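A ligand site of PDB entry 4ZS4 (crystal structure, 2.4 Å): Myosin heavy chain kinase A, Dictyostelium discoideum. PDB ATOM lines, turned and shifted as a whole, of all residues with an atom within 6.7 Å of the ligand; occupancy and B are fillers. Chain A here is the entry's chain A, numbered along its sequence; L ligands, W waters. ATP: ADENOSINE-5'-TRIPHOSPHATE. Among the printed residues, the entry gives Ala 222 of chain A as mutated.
OE2 of Glu 179 is in salt-bridge range of NZ of Lys 111, 2.8 Å away. The side-chain hydroxyl (OG1) of Thr 231 is in hydrogen-bond range of the side-chain carboxylate (OE1) of Glu 179 (2.6 Å). The backbone carbonyl oxygen of Glu 179 sits at hydrogen-bond distance from the backbone NH of Val 109 (2.9 Å). O of Leu 57 sits at hydrogen-bond distance from N of Lys 114. The backbone carbonyl oxygen (O) of Gln 224 lies within hydrogen-bond range of the backbone NH (N) of Thr 231, 2.9 Å away. O of Ala 53 lies within hydrogen-bond range of N of Ala 60 (2.8 Å). O of Ala 60 lies within hydrogen-bond range of N of Phe 52 (2.8 Å). OE2 of Glu 54 is in salt-bridge range of NZ of Lys 114.
OD2 of Asp 232 lies close to O1G of the ligand (2.5 Å). NZ of Lys 111 is in salt-bridge range of O1A of the ligand, at 2.7 Å. An oxygen (O1B) of the ligand lies within hydrogen-bond range of the backbone NH (N) of Arg 58, at 3.0 Å. An oxygen (O1A) of the ligand lies within salt-bridge range of the guanidinium group (NH2) of Arg 58, at 2.7 Å. A nitrogen (N1) of the ligand lies within hydrogen-bond range of the backbone NH (N) of Leu 182, at 2.8 Å. The backbone carbonyl oxygen (O) of Pro 180 is in hydrogen-bond range of a nitrogen (N6) of the ligand, 2.9 Å away. OE1 of Glu 179 lies within hydrogen-bond range of N6 of the ligand (3.0 Å). The backbone NH (N) of Leu 57 sits at hydrogen-bond distance from an oxygen (O1B) of the ligand (3.0 Å). O1G of the ligand lies within salt-bridge range of NZ of Lys 188 (3.0 Å). NE2 of Gln 224 sits at hydrogen-bond distance from O2A of the ligand (3.1 Å).
Water W2 bridges O of Glu 54 (3.0 Å) and O3' of the ligand (3.0 Å). Water W3 bridges O of Asp 232 (2.7 Å) and O1G of the ligand (3.3 Å).
Phe 52 touches the ligand. CB of Ala 53 touches O4' of the ligand (3.5 Å). Glu 54 touches the ligand (C to C5', 3.8 Å). Gly 55 touches the ligand (CA to O2B, 3.0 Å). CB of Ala 56 touches O3G of the ligand (3.6 Å). CB of Ala 60 touches O4' of the ligand, 3.8 Å away. Val 109 touches the ligand (CG2 to N1, 3.8 Å). CD1 of Leu 155 touches N6 of the ligand, 3.8 Å away. Leu 181 touches the ligand. Phe 186 touches the ligand (CD1 to C2', 3.6 Å). CG2 of Thr 231 touches N7 of the ligand (3.8 Å). The nearest printed residue that does not touch the ligand is Ala 222 (5.1 Å).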
ATOM      1  N   PHE A  52      17.640 -37.618   4.470  1.00  0.00           N
ATOM      2  CA  PHE A  52      17.503 -38.122   3.098  1.00  0.00           C
ATOM      3  C   PHE A  52      17.841 -37.069   2.044  1.00  0.00           C
ATOM      4  O   PHE A  52      17.853 -37.390   0.858  1.00  0.00           O
ATOM      5  CB  PHE A  52      16.099 -38.635   2.812  1.00  0.00           C
ATOM      6  CG  PHE A  52      15.055 -37.565   2.726  1.00  0.00           C
ATOM      7  CD1 PHE A  52      14.386 -37.151   3.879  1.00  0.00           C
ATOM      8  CD2 PHE A  52      14.698 -36.984   1.499  1.00  0.00           C
ATOM      9  CE1 PHE A  52      13.396 -36.189   3.829  1.00  0.00           C
ATOM     10  CE2 PHE A  52      13.700 -36.017   1.449  1.00  0.00           C
ATOM     11  CZ  PHE A  52      13.056 -35.619   2.617  1.00  0.00           C
ATOM     12  N   ALA A  53      18.096 -35.833   2.450  1.00  0.00           N
ATOM     13  CA  ALA A  53      18.327 -34.755   1.500  1.00  0.00           C
ATOM     14  C   ALA A  53      18.842 -33.518   2.210  1.00  0.00           C
ATOM     15  O   ALA A  53      18.713 -33.383   3.415  1.00  0.00           O
ATOM     16  CB  ALA A  53      17.062 -34.417   0.726  1.00  0.00           C
ATOM     17  N   GLU A  54      19.478 -32.630   1.453  1.00  0.00           N
ATOM     18  CA  GLU A  54      19.963 -31.386   2.001  1.00  0.00           C
ATOM     19  C   GLU A  54      20.052 -30.347   0.906  1.00  0.00           C
ATOM     20  O   GLU A  54      20.044 -30.679  -0.270  1.00  0.00           O
ATOM     21  CB  GLU A  54      21.321 -31.586   2.676  1.00  0.00           C
ATOM     22  CG  GLU A  54      22.508 -31.876   1.762  1.00  0.00           C
ATOM     23  CD  GLU A  54      23.770 -32.217   2.558  1.00  0.00           C
ATOM     24  OE1 GLU A  54      23.920 -33.382   3.016  1.00  0.00           O
ATOM     25  OE2 GLU A  54      24.615 -31.316   2.712  1.00  0.00           O
ATOM     26  N   GLY A  55      20.112 -29.088   1.308  1.00  0.00           N
ATOM     27  CA  GLY A  55      20.280 -27.975   0.387  1.00  0.00           C
ATOM     28  C   GLY A  55      21.272 -27.023   0.975  1.00  0.00           C
ATOM     29  O   GLY A  55      22.035 -27.390   1.869  1.00  0.00           O
ATOM     30  N   ALA A  56      21.246 -25.776   0.500  1.00  0.00           N
ATOM     31  CA  ALA A  56      22.199 -24.762   0.942  1.00  0.00           C
ATOM     32  C   ALA A  56      22.279 -24.628   2.476  1.00  0.00           C
ATOM     33  O   ALA A  56      23.366 -24.558   3.035  1.00  0.00           O
ATOM     34  CB  ALA A  56      21.870 -23.405   0.312  1.00  0.00           C
ATOM     35  N   LEU A  57      21.119 -24.621   3.139  1.00  0.00           N
ATOM     36  CA  LEU A  57      21.023 -24.306   4.573  1.00  0.00           C
ATOM     37  C   LEU A  57      20.624 -25.457   5.499  1.00  0.00           C
ATOM     38  O   LEU A  57      21.023 -25.489   6.652  1.00  0.00           O
ATOM     39  CB  LEU A  57      20.035 -23.139   4.766  1.00  0.00           C
ATOM     40  CG  LEU A  57      20.498 -21.746   4.288  1.00  0.00           C
ATOM     41  CD1 LEU A  57      19.395 -20.700   4.401  1.00  0.00           C
ATOM     42  CD2 LEU A  57      21.721 -21.296   5.084  1.00  0.00           C
ATOM     43  N   ARG A  58      19.830 -26.412   5.006  1.00  0.00           N
ATOM     44  CA  ARG A  58      19.166 -27.368   5.885  1.00  0.00           C
ATOM     45  C   ARG A  58      19.339 -28.818   5.453  1.00  0.00           C
ATOM     46  O   ARG A  58      19.670 -29.083   4.291  1.00  0.00           O
ATOM     47  CB  ARG A  58      17.675 -27.014   5.979  1.00  0.00           C
ATOM     48  CG  ARG A  58      17.425 -25.598   6.505  1.00  0.00           C
ATOM     49  CD  ARG A  58      15.955 -25.264   6.699  1.00  0.00           C
ATOM     50  NE  ARG A  58      15.243 -25.135   5.427  1.00  0.00           N
ATOM     51  CZ  ARG A  58      13.911 -25.022   5.321  1.00  0.00           C
ATOM     52  NH1 ARG A  58      13.146 -24.983   6.412  1.00  0.00           N
ATOM     53  NH2 ARG A  58      13.352 -24.937   4.123  1.00  0.00           N
ATOM     54  N   GLU A  59      19.122 -29.730   6.385  1.00  0.00           N
ATOM     55  CA  GLU A  59      18.995 -31.160   6.062  1.00  0.00           C
ATOM     56  C   GLU A  59      17.572 -31.605   6.368  1.00  0.00           C
ATOM     57  O   GLU A  59      16.959 -31.120   7.325  1.00  0.00           O
ATOM     58  CB  GLU A  59      19.942 -31.997   6.907  1.00  0.00           C
ATOM     59  CG  GLU A  59      21.415 -31.732   6.666  1.00  0.00           C
ATOM     60  CD  GLU A  59      22.314 -32.097   7.843  1.00  0.00           C
ATOM     61  OE1 GLU A  59      21.801 -32.371   8.965  1.00  0.00           O
ATOM     62  OE2 GLU A  59      23.551 -32.126   7.612  1.00  0.00           O
ATOM     63  N   ALA A  60      17.089 -32.570   5.599  1.00  0.00           N
ATOM     64  CA  ALA A  60      15.735 -33.059   5.720  1.00  0.00           C
ATOM     65  C   ALA A  60      15.740 -34.515   6.132  1.00  0.00           C
ATOM     66  O   ALA A  60      16.527 -35.291   5.613  1.00  0.00           O
ATOM     67  CB  ALA A  60      15.005 -32.888   4.403  1.00  0.00           C
ATOM     68  N   HIS A  62      13.271 -38.076   7.092  1.00  0.00           N
ATOM     69  CA  HIS A  62      11.993 -38.764   7.178  1.00  0.00           C
ATOM     70  C   HIS A  62      11.605 -38.949   8.631  1.00  0.00           C
ATOM     71  O   HIS A  62      12.463 -39.241   9.490  1.00  0.00           O
ATOM     72  CB  HIS A  62      12.041 -40.104   6.485  1.00  0.00           C
ATOM     73  CG  HIS A  62      12.147 -39.975   5.013  1.00  0.00           C
ATOM     74  ND1 HIS A  62      11.141 -39.430   4.251  1.00  0.00           N
ATOM     75  CD2 HIS A  62      13.150 -40.275   4.169  1.00  0.00           C
ATOM     76  CE1 HIS A  62      11.512 -39.429   2.982  1.00  0.00           C
ATOM     77  NE2 HIS A  62      12.724 -39.933   2.914  1.00  0.00           N
ATOM     78  N   VAL A 109       8.174 -34.685   7.023  1.00  0.00           N
ATOM     79  CA  VAL A 109       9.566 -34.277   6.909  1.00  0.00           C
ATOM     80  C   VAL A 109       9.955 -33.298   8.009  1.00  0.00           C
ATOM     81  O   VAL A 109       9.184 -32.422   8.381  1.00  0.00           O
ATOM     82  CB  VAL A 109       9.806 -33.608   5.543  1.00  0.00           C
ATOM     83  CG1 VAL A 109      11.216 -33.060   5.434  1.00  0.00           C
ATOM     84  CG2 VAL A 109       9.518 -34.603   4.431  1.00  0.00           C
ATOM     85  N   LYS A 111      13.126 -30.689   9.282  1.00  0.00           N
ATOM     86  CA  LYS A 111      14.288 -29.996   8.760  1.00  0.00           C
ATOM     87  C   LYS A 111      15.086 -29.305   9.843  1.00  0.00           C
ATOM     88  O   LYS A 111      14.544 -28.565  10.649  1.00  0.00           O
ATOM     89  CB  LYS A 111      13.865 -28.954   7.712  1.00  0.00           C
ATOM     90  CG  LYS A 111      13.157 -29.577   6.524  1.00  0.00           C
ATOM     91  CD  LYS A 111      12.741 -28.524   5.524  1.00  0.00           C
ATOM     92  CE  LYS A 111      12.157 -29.183   4.311  1.00  0.00           C
ATOM     93  NZ  LYS A 111      11.530 -28.207   3.389  1.00  0.00           N
ATOM     94  N   TYR A 113      18.637 -26.867  10.596  1.00  0.00           N
ATOM     95  CA  TYR A 113      19.675 -26.040  10.048  1.00  0.00           C
ATOM     96  C   TYR A 113      20.998 -26.758  10.245  1.00  0.00           C
ATOM     97  O   TYR A 113      21.190 -27.446  11.236  1.00  0.00           O
ATOM     98  CB  TYR A 113      19.727 -24.685  10.747  1.00  0.00           C
ATOM     99  CG  TYR A 113      18.758 -23.691  10.179  1.00  0.00           C
ATOM    100  CD1 TYR A 113      18.864 -23.263   8.854  1.00  0.00           C
ATOM    101  CD2 TYR A 113      17.731 -23.160  10.952  1.00  0.00           C
ATOM    102  CE1 TYR A 113      17.976 -22.342   8.332  1.00  0.00           C
ATOM    103  CE2 TYR A 113      16.855 -22.240  10.422  1.00  0.00           C
ATOM    104  CZ  TYR A 113      16.986 -21.829   9.111  1.00  0.00           C
ATOM    105  OH  TYR A 113      16.113 -20.921   8.575  1.00  0.00           O
ATOM    106  N   LYS A 114      21.899 -26.616   9.269  1.00  0.00           N
ATOM    107  CA  LYS A 114      23.251 -27.132   9.415  1.00  0.00           C
ATOM    108  C   LYS A 114      24.112 -26.245  10.331  1.00  0.00           C
ATOM    109  O   LYS A 114      23.775 -25.082  10.583  1.00  0.00           O
ATOM    110  CB  LYS A 114      23.915 -27.243   8.052  1.00  0.00           C
ATOM    111  CG  LYS A 114      23.443 -28.457   7.287  1.00  0.00           C
ATOM    112  CD  LYS A 114      24.173 -28.613   5.954  1.00  0.00           C
ATOM    113  CE  LYS A 114      23.635 -27.673   4.888  1.00  0.00           C
ATOM    114  NZ  LYS A 114      23.811 -28.260   3.541  1.00  0.00           N
ATOM    115  N   LEU A 155       2.603 -26.067   1.004  1.00  0.00           N
ATOM    116  CA  LEU A 155       2.430 -26.917   2.163  1.00  0.00           C
ATOM    117  C   LEU A 155       2.358 -26.111   3.467  1.00  0.00           C
ATOM    118  O   LEU A 155       2.927 -25.029   3.598  1.00  0.00           O
ATOM    119  CB  LEU A 155       3.624 -27.872   2.278  1.00  0.00           C
ATOM    120  CG  LEU A 155       3.848 -28.904   1.187  1.00  0.00           C
ATOM    121  CD1 LEU A 155       5.082 -29.735   1.564  1.00  0.00           C
ATOM    122  CD2 LEU A 155       2.630 -29.783   1.018  1.00  0.00           C
ATOM    123  N   GLU A 179       7.063 -30.344   7.990  1.00  0.00           N
ATOM    124  CA  GLU A 179       6.084 -30.148   6.949  1.00  0.00           C
ATOM    125  C   GLU A 179       5.690 -31.520   6.366  1.00  0.00           C
ATOM    126  O   GLU A 179       6.365 -32.512   6.588  1.00  0.00           O
ATOM    127  CB  GLU A 179       6.677 -29.241   5.864  1.00  0.00           C
ATOM    128  CG  GLU A 179       7.955 -29.753   5.238  1.00  0.00           C
ATOM    129  CD  GLU A 179       8.619 -28.731   4.323  1.00  0.00           C
ATOM    130  OE1 GLU A 179       8.588 -28.912   3.076  1.00  0.00           O
ATOM    131  OE2 GLU A 179       9.207 -27.749   4.848  1.00  0.00           O
ATOM    132  N   PRO A 180       4.603 -31.561   5.583  1.00  0.00           N
ATOM    133  CA  PRO A 180       4.199 -32.800   4.938  1.00  0.00           C
ATOM    134  C   PRO A 180       5.255 -33.329   3.978  1.00  0.00           C
ATOM    135  O   PRO A 180       6.113 -32.588   3.542  1.00  0.00           O
ATOM    136  CB  PRO A 180       2.937 -32.408   4.186  1.00  0.00           C
ATOM    137  CG  PRO A 180       2.385 -31.268   4.981  1.00  0.00           C
ATOM    138  CD  PRO A 180       3.611 -30.491   5.344  1.00  0.00           C
ATOM    139  N   LEU A 181       5.189 -34.611   3.685  1.00  0.00           N
ATOM    140  CA  LEU A 181       6.146 -35.238   2.756  1.00  0.00           C
ATOM    141  C   LEU A 181       5.646 -35.014   1.355  1.00  0.00           C
ATOM    142  O   LEU A 181       4.502 -35.285   1.077  1.00  0.00           O
ATOM    143  CB  LEU A 181       6.240 -36.745   3.039  1.00  0.00           C
ATOM    144  CG  LEU A 181       7.071 -37.571   2.053  1.00  0.00           C
ATOM    145  CD1 LEU A 181       8.559 -37.216   2.130  1.00  0.00           C
ATOM    146  CD2 LEU A 181       6.879 -39.058   2.324  1.00  0.00           C
ATOM    147  N   LEU A 182       6.478 -34.497   0.488  1.00  0.00           N
ATOM    148  CA  LEU A 182       6.134 -34.448  -0.934  1.00  0.00           C
ATOM    149  C   LEU A 182       6.580 -35.726  -1.637  1.00  0.00           C
ATOM    150  O   LEU A 182       7.769 -36.094  -1.567  1.00  0.00           O
ATOM    151  CB  LEU A 182       6.802 -33.270  -1.623  1.00  0.00           C
ATOM    152  CG  LEU A 182       6.250 -31.906  -1.250  1.00  0.00           C
ATOM    153  CD1 LEU A 182       7.071 -30.822  -1.911  1.00  0.00           C
ATOM    154  CD2 LEU A 182       4.788 -31.755  -1.637  1.00  0.00           C
ATOM    155  N   VAL A 183       5.656 -36.394  -2.308  1.00  0.00           N
ATOM    156  CA  VAL A 183       6.018 -37.552  -3.117  1.00  0.00           C
ATOM    157  C   VAL A 183       6.112 -37.193  -4.605  1.00  0.00           C
ATOM    158  O   VAL A 183       5.127 -36.749  -5.215  1.00  0.00           O
ATOM    159  CB  VAL A 183       5.007 -38.714  -2.928  1.00  0.00           C
ATOM    160  CG1 VAL A 183       5.375 -39.884  -3.843  1.00  0.00           C
ATOM    161  CG2 VAL A 183       5.002 -39.172  -1.471  1.00  0.00           C
ATOM    162  N   GLY A 184       7.299 -37.377  -5.174  1.00  0.00           N
ATOM    163  CA  GLY A 184       7.529 -37.119  -6.582  1.00  0.00           C
ATOM    164  C   GLY A 184       8.887 -36.510  -6.844  1.00  0.00           C
ATOM    165  O   GLY A 184       9.780 -36.525  -5.987  1.00  0.00           O
ATOM    166  N   PHE A 186      11.172 -33.589  -6.979  1.00  0.00           N
ATOM    167  CA  PHE A 186      11.293 -32.278  -6.401  1.00  0.00           C
ATOM    168  C   PHE A 186      12.095 -31.390  -7.332  1.00  0.00           C
ATOM    169  O   PHE A 186      13.238 -31.710  -7.649  1.00  0.00           O
ATOM    170  CB  PHE A 186      11.983 -32.385  -5.037  1.00  0.00           C
ATOM    171  CG  PHE A 186      11.868 -31.149  -4.188  1.00  0.00           C
ATOM    172  CD1 PHE A 186      12.690 -30.054  -4.408  1.00  0.00           C
ATOM    173  CD2 PHE A 186      10.929 -31.092  -3.145  1.00  0.00           C
ATOM    174  CE1 PHE A 186      12.576 -28.933  -3.604  1.00  0.00           C
ATOM    175  CE2 PHE A 186      10.818 -29.966  -2.348  1.00  0.00           C
ATOM    176  CZ  PHE A 186      11.652 -28.889  -2.574  1.00  0.00           C
ATOM    177  N   LYS A 188      13.195 -27.170  -8.409  1.00  0.00           N
ATOM    178  CA  LYS A 188      13.309 -25.774  -8.074  1.00  0.00           C
ATOM    179  C   LYS A 188      13.115 -24.947  -9.335  1.00  0.00           C
ATOM    180  O   LYS A 188      13.832 -25.145 -10.293  1.00  0.00           O
ATOM    181  CB  LYS A 188      14.673 -25.505  -7.461  1.00  0.00           C
ATOM    182  CG  LYS A 188      14.843 -24.081  -6.954  1.00  0.00           C
ATOM    183  CD  LYS A 188      16.249 -23.808  -6.408  1.00  0.00           C
ATOM    184  CE  LYS A 188      16.242 -22.835  -5.211  1.00  0.00           C
ATOM    185  NZ  LYS A 188      16.438 -23.560  -3.910  1.00  0.00           N
ATOM    186  N   ALA A 222      11.811 -18.297  -4.932  1.00  0.00           N
ATOM    187  CA  ALA A 222      12.249 -19.648  -4.551  1.00  0.00           C
ATOM    188  C   ALA A 222      11.090 -20.645  -4.612  1.00  0.00           C
ATOM    189  O   ALA A 222      10.882 -21.479  -3.702  1.00  0.00           O
ATOM    190  CB  ALA A 222      12.911 -19.659  -3.167  1.00  0.00           C
ATOM    191  N   GLN A 224       9.389 -23.809  -5.514  1.00  0.00           N
ATOM    192  CA  GLN A 224      10.019 -25.114  -5.584  1.00  0.00           C
ATOM    193  C   GLN A 224       9.155 -26.155  -4.918  1.00  0.00           C
ATOM    194  O   GLN A 224       8.483 -25.880  -3.928  1.00  0.00           O
ATOM    195  CB  GLN A 224      11.415 -25.082  -4.963  1.00  0.00           C
ATOM    196  CG  GLN A 224      11.479 -25.218  -3.451  1.00  0.00           C
ATOM    197  CD  GLN A 224      12.767 -24.684  -2.838  1.00  0.00           C
ATOM    198  OE1 GLN A 224      12.938 -23.465  -2.674  1.00  0.00           O
ATOM    199  NE2 GLN A 224      13.629 -25.575  -2.424  1.00  0.00           N
ATOM    200  N   VAL A 226       7.018 -30.257  -5.875  1.00  0.00           N
ATOM    201  CA  VAL A 226       6.667 -31.331  -6.762  1.00  0.00           C
ATOM    202  C   VAL A 226       5.424 -30.864  -7.458  1.00  0.00           C
ATOM    203  O   VAL A 226       4.425 -30.612  -6.794  1.00  0.00           O
ATOM    204  CB  VAL A 226       6.340 -32.623  -5.990  1.00  0.00           C
ATOM    205  CG1 VAL A 226       5.758 -33.671  -6.922  1.00  0.00           C
ATOM    206  CG2 VAL A 226       7.579 -33.161  -5.315  1.00  0.00           C
ATOM    207  N   THR A 231       7.036 -25.636  -1.412  1.00  0.00           N
ATOM    208  CA  THR A 231       7.531 -25.486  -0.049  1.00  0.00           C
ATOM    209  C   THR A 231       8.829 -24.689  -0.083  1.00  0.00           C
ATOM    210  O   THR A 231       9.307 -24.346  -1.152  1.00  0.00           O
ATOM    211  CB  THR A 231       7.724 -26.856   0.634  1.00  0.00           C
ATOM    212  OG1 THR A 231       7.903 -26.676   2.029  1.00  0.00           O
ATOM    213  CG2 THR A 231       8.913 -27.632   0.069  1.00  0.00           C
ATOM    214  N   ASP A 232       9.348 -24.347   1.081  1.00  0.00           N
ATOM    215  CA  ASP A 232      10.565 -23.504   1.189  1.00  0.00           C
ATOM    216  C   ASP A 232      10.597 -22.257   0.284  1.00  0.00           C
ATOM    217  O   ASP A 232      11.601 -21.972  -0.349  1.00  0.00           O
ATOM    218  CB  ASP A 232      11.805 -24.390   0.924  1.00  0.00           C
ATOM    219  CG  ASP A 232      13.131 -23.665   1.151  1.00  0.00           C
ATOM    220  OD1 ASP A 232      13.248 -22.865   2.124  1.00  0.00           O
ATOM    221  OD2 ASP A 232      14.070 -23.883   0.353  1.00  0.00           O
HETATM  222  PG  ATP L   1      17.209 -23.783  -0.339  1.00  0.00           P
HETATM  223  O1G ATP L   1      16.059 -23.028  -0.978  1.00  0.00           O
HETATM  224  O2G ATP L   1      17.624 -25.004  -1.124  1.00  0.00           O
HETATM  225  O3G ATP L   1      18.368 -22.878   0.058  1.00  0.00           O
HETATM  226  PB  ATP L   1      17.235 -25.659   1.730  1.00  0.00           P
HETATM  227  O1B ATP L   1      18.230 -25.239   2.779  1.00  0.00           O
HETATM  228  O2B ATP L   1      17.673 -26.494   0.535  1.00  0.00           O
HETATM  229  O3B ATP L   1      16.584 -24.329   1.080  1.00  0.00           O
HETATM  230  PA  ATP L   1      14.903 -27.260   1.528  1.00  0.00           P
HETATM  231  O1A ATP L   1      13.672 -26.963   2.387  1.00  0.00           O
HETATM  232  O2A ATP L   1      14.847 -26.966   0.041  1.00  0.00           O
HETATM  233  O3A ATP L   1      16.076 -26.543   2.364  1.00  0.00           O
HETATM  234  O5' ATP L   1      15.219 -28.840   1.733  1.00  0.00           O
HETATM  235  C5' ATP L   1      16.347 -29.482   1.158  1.00  0.00           C
HETATM  236  C4' ATP L   1      15.918 -30.610   0.239  1.00  0.00           C
HETATM  237  O4' ATP L   1      14.992 -31.553   0.820  1.00  0.00           O
HETATM  238  C3' ATP L   1      15.228 -30.071  -0.998  1.00  0.00           C
HETATM  239  O3' ATP L   1      16.215 -29.550  -1.875  1.00  0.00           O
HETATM  240  C2' ATP L   1      14.485 -31.289  -1.489  1.00  0.00           C
HETATM  241  O2' ATP L   1      15.403 -32.176  -2.140  1.00  0.00           O
HETATM  242  C1' ATP L   1      14.049 -31.953  -0.191  1.00  0.00           C
HETATM  243  N9  ATP L   1      12.707 -31.610   0.350  1.00  0.00           N
HETATM  244  C8  ATP L   1      12.396 -30.437   0.977  1.00  0.00           C
HETATM  245  N7  ATP L   1      11.102 -30.446   1.386  1.00  0.00           N
HETATM  246  C5  ATP L   1      10.596 -31.630   1.069  1.00  0.00           C
HETATM  247  C6  ATP L   1       9.302 -32.271   1.265  1.00  0.00           C
HETATM  248  N6  ATP L   1       8.337 -31.596   1.877  1.00  0.00           N
HETATM  249  N1  ATP L   1       9.119 -33.530   0.779  1.00  0.00           N
HETATM  250  C2  ATP L   1      10.126 -34.184   0.162  1.00  0.00           C
HETATM  251  N3  ATP L   1      11.345 -33.657  -0.039  1.00  0.00           N
HETATM  252  C4  ATP L   1      11.639 -32.403   0.384  1.00  0.00           C
HETATM  253  O   HOH W   1      14.218 -34.152  -3.189  1.00  0.00           O
HETATM  254  O   HOH W   2      18.670 -30.985  -2.973  1.00  0.00           O
HETATM  255  O   HOH W   3      13.925 -20.740   0.155  1.00  0.00           O
